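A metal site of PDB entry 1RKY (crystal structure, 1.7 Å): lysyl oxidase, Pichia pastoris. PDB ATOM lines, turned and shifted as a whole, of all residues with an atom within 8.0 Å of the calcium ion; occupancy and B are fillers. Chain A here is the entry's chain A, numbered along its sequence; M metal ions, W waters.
The backbone carbonyl oxygen of Asp 643 lies within hydrogen-bond range of the backbone NH of His 607 (2.8 Å). The side-chain amino group (NZ) of Lys 65 is in salt-bridge range of the side-chain carboxylate (OD2) of Asp 499. The backbone carbonyl oxygen (O) of Glu 334 lies within hydrogen-bond range of the backbone NH (N) of Asp 497 (2.8 Å). N of Asp 499 sits at hydrogen-bond distance from O of Ile 331 (2.9 Å). The backbone carbonyl oxygen of Asp 497 is in hydrogen-bond range of the backbone NH of Tyr 333. The side-chain carboxylate (OD2) of Asp 497 lies within salt-bridge range of the side-chain amino group (NZ) of Lys 65 (2.7 Å). NZ of Lys 65 is in salt-bridge range of OD2 of Asp 643, 2.7 Å away.
Lys 65 touches the calcium ion. Six residues have an atom within 4 Å of the calcium ion: Lys 65, Asp 497, Leu 498, Asp 499, Asp 643 and Ile 644.
The calcium ion is bound by the side-chain carboxylate of Asp 499 (2.3 Å), the backbone carbonyl oxygen of Ile 644 (2.3 Å), the side-chain carboxylate of Asp 643 (2.3 Å), the backbone carbonyl oxygen of Leu 498 (2.3 Å), the side-chain carboxylate of Asp 497 (2.4 Å) and water W1 (2.5 Å). The calcium ion has six donor atoms within binding distance.
Water W1 lies within hydrogen-bond range of the backbone carbonyl oxygen (O) of Thr 503 (2.6 Å), the side-chain amide oxygen (OD1) of Asn 505 (2.7 Å) and the backbone NH (N) of Ile 644 (3.1 Å).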
ATOM      1  N   LYS A  65     -20.153  12.752   5.848  1.00  0.00           N
ATOM      2  CA  LYS A  65     -21.249  13.288   6.617  1.00  0.00           C
ATOM      3  C   LYS A  65     -22.220  12.239   7.142  1.00  0.00           C
ATOM      4  O   LYS A  65     -22.601  12.295   8.296  1.00  0.00           O
ATOM      5  CB  LYS A  65     -22.023  14.317   5.814  1.00  0.00           C
ATOM      6  CG  LYS A  65     -23.088  15.011   6.617  1.00  0.00           C
ATOM      7  CD  LYS A  65     -23.579  16.275   5.893  1.00  0.00           C
ATOM      8  CE  LYS A  65     -24.679  16.961   6.686  1.00  0.00           C
ATOM      9  NZ  LYS A  65     -25.158  18.144   5.885  1.00  0.00           N
ATOM     10  N   ILE A 331     -27.934  23.246  13.932  1.00  0.00           N
ATOM     11  CA  ILE A 331     -28.295  24.188  12.859  1.00  0.00           C
ATOM     12  C   ILE A 331     -27.295  24.166  11.726  1.00  0.00           C
ATOM     13  O   ILE A 331     -27.699  24.338  10.576  1.00  0.00           O
ATOM     14  CB  ILE A 331     -28.455  25.626  13.417  1.00  0.00           C
ATOM     15  CG1 ILE A 331     -29.524  25.662  14.499  1.00  0.00           C
ATOM     16  CG2 ILE A 331     -28.834  26.629  12.308  1.00  0.00           C
ATOM     17  CD1 ILE A 331     -29.398  26.836  15.404  1.00  0.00           C
ATOM     18  N   VAL A 332     -26.011  23.951  12.024  1.00  0.00           N
ATOM     19  CA  VAL A 332     -24.970  23.888  10.993  1.00  0.00           C
ATOM     20  C   VAL A 332     -24.124  22.657  11.213  1.00  0.00           C
ATOM     21  O   VAL A 332     -23.528  22.502  12.269  1.00  0.00           O
ATOM     22  CB  VAL A 332     -24.081  25.186  10.979  1.00  0.00           C
ATOM     23  CG1 VAL A 332     -22.944  25.077   9.959  1.00  0.00           C
ATOM     24  CG2 VAL A 332     -24.930  26.467  10.739  1.00  0.00           C
ATOM     25  N   TYR A 333     -24.031  21.789  10.208  1.00  0.00           N
ATOM     26  CA  TYR A 333     -23.118  20.653  10.292  1.00  0.00           C
ATOM     27  C   TYR A 333     -21.649  21.045  10.230  1.00  0.00           C
ATOM     28  O   TYR A 333     -20.816  20.572  11.007  1.00  0.00           O
ATOM     29  CB  TYR A 333     -23.445  19.589   9.232  1.00  0.00           C
ATOM     30  CG  TYR A 333     -22.421  18.486   9.259  1.00  0.00           C
ATOM     31  CD1 TYR A 333     -22.414  17.555  10.310  1.00  0.00           C
ATOM     32  CD2 TYR A 333     -21.445  18.397   8.291  1.00  0.00           C
ATOM     33  CE1 TYR A 333     -21.456  16.576  10.370  1.00  0.00           C
ATOM     34  CE2 TYR A 333     -20.448  17.396   8.348  1.00  0.00           C
ATOM     35  CZ  TYR A 333     -20.477  16.497   9.411  1.00  0.00           C
ATOM     36  OH  TYR A 333     -19.529  15.509   9.475  1.00  0.00           O
ATOM     37  N   GLU A 334     -21.320  21.896   9.258  1.00  0.00           N
ATOM     38  CA  GLU A 334     -19.949  22.312   9.018  1.00  0.00           C
ATOM     39  C   GLU A 334     -19.984  23.792   8.622  1.00  0.00           C
ATOM     40  O   GLU A 334     -20.764  24.171   7.732  1.00  0.00           O
ATOM     41  CB  GLU A 334     -19.336  21.491   7.888  1.00  0.00           C
ATOM     42  CG  GLU A 334     -17.956  21.985   7.467  1.00  0.00           C
ATOM     43  CD  GLU A 334     -17.270  21.210   6.324  1.00  0.00           C
ATOM     44  OE1 GLU A 334     -16.116  21.598   6.007  1.00  0.00           O
ATOM     45  OE2 GLU A 334     -17.871  20.288   5.722  1.00  0.00           O
ATOM     46  N   VAL A 496     -20.925  26.818   4.213  1.00  0.00           N
ATOM     47  CA  VAL A 496     -21.909  26.988   5.268  1.00  0.00           C
ATOM     48  C   VAL A 496     -22.928  25.875   5.073  1.00  0.00           C
ATOM     49  O   VAL A 496     -23.893  26.046   4.336  1.00  0.00           O
ATOM     50  CB  VAL A 496     -22.598  28.382   5.209  1.00  0.00           C
ATOM     51  CG1 VAL A 496     -23.555  28.551   6.319  1.00  0.00           C
ATOM     52  CG2 VAL A 496     -21.524  29.500   5.250  1.00  0.00           C
ATOM     53  N   ASP A 497     -22.675  24.745   5.717  1.00  0.00           N
ATOM     54  CA  ASP A 497     -23.558  23.584   5.593  1.00  0.00           C
ATOM     55  C   ASP A 497     -24.652  23.672   6.652  1.00  0.00           C
ATOM     56  O   ASP A 497     -24.635  23.000   7.681  1.00  0.00           O
ATOM     57  CB  ASP A 497     -22.762  22.295   5.703  1.00  0.00           C
ATOM     58  CG  ASP A 497     -23.577  21.079   5.409  1.00  0.00           C
ATOM     59  OD1 ASP A 497     -24.771  21.247   5.072  1.00  0.00           O
ATOM     60  OD2 ASP A 497     -23.106  19.930   5.562  1.00  0.00           O
ATOM     61  N   LEU A 498     -25.612  24.538   6.381  1.00  0.00           N
ATOM     62  CA  LEU A 498     -26.809  24.659   7.180  1.00  0.00           C
ATOM     63  C   LEU A 498     -27.665  23.406   6.994  1.00  0.00           C
ATOM     64  O   LEU A 498     -27.810  22.942   5.891  1.00  0.00           O
ATOM     65  CB  LEU A 498     -27.626  25.865   6.729  1.00  0.00           C
ATOM     66  CG  LEU A 498     -27.182  27.227   7.312  1.00  0.00           C
ATOM     67  CD1 LEU A 498     -27.640  28.367   6.388  1.00  0.00           C
ATOM     68  CD2 LEU A 498     -27.715  27.464   8.675  1.00  0.00           C
ATOM     69  N   ASP A 499     -28.157  22.886   8.115  1.00  0.00           N
ATOM     70  CA  ASP A 499     -29.141  21.794   8.151  1.00  0.00           C
ATOM     71  C   ASP A 499     -30.259  22.262   9.063  1.00  0.00           C
ATOM     72  O   ASP A 499     -30.277  21.975  10.264  1.00  0.00           O
ATOM     73  CB  ASP A 499     -28.532  20.521   8.752  1.00  0.00           C
ATOM     74  CG  ASP A 499     -27.508  19.829   7.889  1.00  0.00           C
ATOM     75  OD1 ASP A 499     -27.352  20.077   6.632  1.00  0.00           O
ATOM     76  OD2 ASP A 499     -26.834  18.903   8.430  1.00  0.00           O
ATOM     77  N   VAL A 500     -31.210  23.004   8.515  1.00  0.00           N
ATOM     78  CA  VAL A 500     -32.226  23.665   9.280  1.00  0.00           C
ATOM     79  C   VAL A 500     -33.399  22.686   9.494  1.00  0.00           C
ATOM     80  O   VAL A 500     -34.059  22.255   8.547  1.00  0.00           O
ATOM     81  CB  VAL A 500     -32.741  24.950   8.544  1.00  0.00           C
ATOM     82  CG1 VAL A 500     -33.831  25.656   9.397  1.00  0.00           C
ATOM     83  CG2 VAL A 500     -31.598  25.900   8.245  1.00  0.00           C
ATOM     84  N   GLY A 502     -33.146  19.534  10.341  1.00  0.00           N
ATOM     85  CA  GLY A 502     -32.676  18.346   9.621  1.00  0.00           C
ATOM     86  C   GLY A 502     -31.921  18.637   8.349  1.00  0.00           C
ATOM     87  O   GLY A 502     -31.752  19.815   7.990  1.00  0.00           O
ATOM     88  N   THR A 503     -31.426  17.598   7.676  1.00  0.00           N
ATOM     89  CA  THR A 503     -30.655  17.799   6.440  1.00  0.00           C
ATOM     90  C   THR A 503     -31.521  18.189   5.252  1.00  0.00           C
ATOM     91  O   THR A 503     -31.067  18.914   4.365  1.00  0.00           O
ATOM     92  CB  THR A 503     -29.850  16.534   6.053  1.00  0.00           C
ATOM     93  OG1 THR A 503     -30.739  15.395   6.036  1.00  0.00           O
ATOM     94  CG2 THR A 503     -28.792  16.211   7.043  1.00  0.00           C
ATOM     95  N   LYS A 504     -32.753  17.652   5.194  1.00  0.00           N
ATOM     96  CA  LYS A 504     -33.630  17.872   4.040  1.00  0.00           C
ATOM     97  C   LYS A 504     -34.210  19.290   4.082  1.00  0.00           C
ATOM     98  O   LYS A 504     -35.038  19.600   4.910  1.00  0.00           O
ATOM     99  CB  LYS A 504     -34.760  16.828   4.007  1.00  0.00           C
ATOM    100  CG  LYS A 504     -35.459  16.756   2.709  1.00  0.00           C
ATOM    101  CD  LYS A 504     -36.620  15.774   2.729  1.00  0.00           C
ATOM    102  CE  LYS A 504     -37.367  15.755   1.404  1.00  0.00           C
ATOM    103  NZ  LYS A 504     -38.688  15.034   1.499  1.00  0.00           N
ATOM    104  N   ASN A 505     -33.733  20.134   3.178  1.00  0.00           N
ATOM    105  CA  ASN A 505     -34.044  21.545   3.176  1.00  0.00           C
ATOM    106  C   ASN A 505     -34.472  22.016   1.763  1.00  0.00           C
ATOM    107  O   ASN A 505     -34.425  21.271   0.753  1.00  0.00           O
ATOM    108  CB  ASN A 505     -32.762  22.374   3.588  1.00  0.00           C
ATOM    109  CG  ASN A 505     -32.359  22.235   5.054  1.00  0.00           C
ATOM    110  OD1 ASN A 505     -31.307  22.777   5.433  1.00  0.00           O
ATOM    111  ND2 ASN A 505     -33.143  21.550   5.890  1.00  0.00           N
ATOM    112  N   ILE A 557     -32.649  29.435   4.013  1.00  0.00           N
ATOM    113  CA  ILE A 557     -32.587  27.988   3.970  1.00  0.00           C
ATOM    114  C   ILE A 557     -33.684  27.483   4.909  1.00  0.00           C
ATOM    115  O   ILE A 557     -33.698  27.787   6.072  1.00  0.00           O
ATOM    116  CB  ILE A 557     -31.208  27.479   4.392  1.00  0.00           C
ATOM    117  CG1 ILE A 557     -30.147  28.076   3.455  1.00  0.00           C
ATOM    118  CG2 ILE A 557     -31.172  25.963   4.346  1.00  0.00           C
ATOM    119  CD1 ILE A 557     -30.285  27.718   1.993  1.00  0.00           C
ATOM    120  N   THR A 605     -25.513  24.437  -3.468  1.00  0.00           N
ATOM    121  CA  THR A 605     -25.279  23.124  -4.081  1.00  0.00           C
ATOM    122  C   THR A 605     -25.869  22.036  -3.216  1.00  0.00           C
ATOM    123  O   THR A 605     -26.140  22.236  -2.013  1.00  0.00           O
ATOM    124  CB  THR A 605     -23.768  22.830  -4.299  1.00  0.00           C
ATOM    125  OG1 THR A 605     -23.086  22.712  -3.049  1.00  0.00           O
ATOM    126  CG2 THR A 605     -23.062  23.921  -5.064  1.00  0.00           C
ATOM    127  N   LYS A 606     -26.057  20.869  -3.828  1.00  0.00           N
ATOM    128  CA  LYS A 606     -26.449  19.668  -3.112  1.00  0.00           C
ATOM    129  C   LYS A 606     -25.209  19.099  -2.457  1.00  0.00           C
ATOM    130  O   LYS A 606     -24.163  18.919  -3.091  1.00  0.00           O
ATOM    131  CB  LYS A 606     -27.043  18.651  -4.096  1.00  0.00           C
ATOM    132  CG  LYS A 606     -27.277  17.269  -3.538  1.00  0.00           C
ATOM    133  CD  LYS A 606     -28.003  16.419  -4.604  1.00  0.00           C
ATOM    134  CE  LYS A 606     -27.950  14.927  -4.277  1.00  0.00           C
ATOM    135  NZ  LYS A 606     -28.622  14.124  -5.349  1.00  0.00           N
ATOM    136  N   HIS A 607     -25.323  18.829  -1.161  1.00  0.00           N
ATOM    137  CA  HIS A 607     -24.215  18.300  -0.400  1.00  0.00           C
ATOM    138  C   HIS A 607     -23.734  16.983  -0.966  1.00  0.00           C
ATOM    139  O   HIS A 607     -24.544  16.106  -1.311  1.00  0.00           O
ATOM    140  CB  HIS A 607     -24.610  18.059   1.061  1.00  0.00           C
ATOM    141  CG  HIS A 607     -23.476  17.538   1.867  1.00  0.00           C
ATOM    142  ND1 HIS A 607     -23.142  16.196   1.894  1.00  0.00           N
ATOM    143  CD2 HIS A 607     -22.512  18.189   2.570  1.00  0.00           C
ATOM    144  CE1 HIS A 607     -22.036  16.047   2.607  1.00  0.00           C
ATOM    145  NE2 HIS A 607     -21.642  17.230   3.037  1.00  0.00           N
ATOM    146  N   GLU A 642     -33.601  18.646  -0.283  1.00  0.00           N
ATOM    147  CA  GLU A 642     -32.276  18.064  -0.433  1.00  0.00           C
ATOM    148  C   GLU A 642     -31.380  18.643   0.691  1.00  0.00           C
ATOM    149  O   GLU A 642     -31.708  19.651   1.300  1.00  0.00           O
ATOM    150  CB  GLU A 642     -31.694  18.354  -1.816  1.00  0.00           C
ATOM    151  CG  GLU A 642     -32.476  17.728  -2.967  1.00  0.00           C
ATOM    152  CD  GLU A 642     -32.459  16.214  -2.975  1.00  0.00           C
ATOM    153  OE1 GLU A 642     -31.637  15.601  -2.269  1.00  0.00           O
ATOM    154  OE2 GLU A 642     -33.270  15.624  -3.706  1.00  0.00           O
ATOM    155  N   ASP A 643     -30.249  17.996   0.929  1.00  0.00           N
ATOM    156  CA  ASP A 643     -29.211  18.524   1.817  1.00  0.00           C
ATOM    157  C   ASP A 643     -28.464  19.593   0.986  1.00  0.00           C
ATOM    158  O   ASP A 643     -27.757  19.249   0.050  1.00  0.00           O
ATOM    159  CB  ASP A 643     -28.249  17.409   2.211  1.00  0.00           C
ATOM    160  CG  ASP A 643     -27.279  17.833   3.299  1.00  0.00           C
ATOM    161  OD1 ASP A 643     -27.192  19.063   3.555  1.00  0.00           O
ATOM    162  OD2 ASP A 643     -26.565  17.005   3.912  1.00  0.00           O
ATOM    163  N   ILE A 644     -28.633  20.849   1.388  1.00  0.00           N
ATOM    164  CA  ILE A 644     -28.083  21.991   0.684  1.00  0.00           C
ATOM    165  C   ILE A 644     -26.861  22.467   1.470  1.00  0.00           C
ATOM    166  O   ILE A 644     -26.806  22.357   2.734  1.00  0.00           O
ATOM    167  CB  ILE A 644     -29.133  23.125   0.603  1.00  0.00           C
ATOM    168  CG1 ILE A 644     -30.355  22.649  -0.215  1.00  0.00           C
ATOM    169  CG2 ILE A 644     -28.536  24.365  -0.042  1.00  0.00           C
ATOM    170  CD1 ILE A 644     -31.557  23.583  -0.175  1.00  0.00           C
ATOM    171  N   VAL A 645     -25.865  22.900   0.721  1.00  0.00           N
ATOM    172  CA  VAL A 645     -24.713  23.637   1.238  1.00  0.00           C
ATOM    173  C   VAL A 645     -24.703  25.032   0.574  1.00  0.00           C
ATOM    174  O   VAL A 645     -24.910  25.142  -0.640  1.00  0.00           O
ATOM    175  CB  VAL A 645     -23.391  22.923   0.877  1.00  0.00           C
ATOM    176  CG1 VAL A 645     -22.139  23.734   1.362  1.00  0.00           C
ATOM    177  CG2 VAL A 645     -23.363  21.514   1.434  1.00  0.00           C
ATOM    178  N   ALA A 646     -24.432  26.076   1.368  1.00  0.00           N
ATOM    179  CA  ALA A 646     -24.307  27.435   0.803  1.00  0.00           C
ATOM    180  C   ALA A 646     -22.802  27.756   0.834  1.00  0.00           C
ATOM    181  O   ALA A 646     -22.142  27.506   1.817  1.00  0.00           O
ATOM    182  CB  ALA A 646     -25.082  28.423   1.630  1.00  0.00           C
HETATM  183 CA    CA M   1     -27.082  21.101   4.630  1.00  0.00          CA
HETATM  184  O   HOH W   1     -29.539  21.075   4.300  1.00  0.00           O
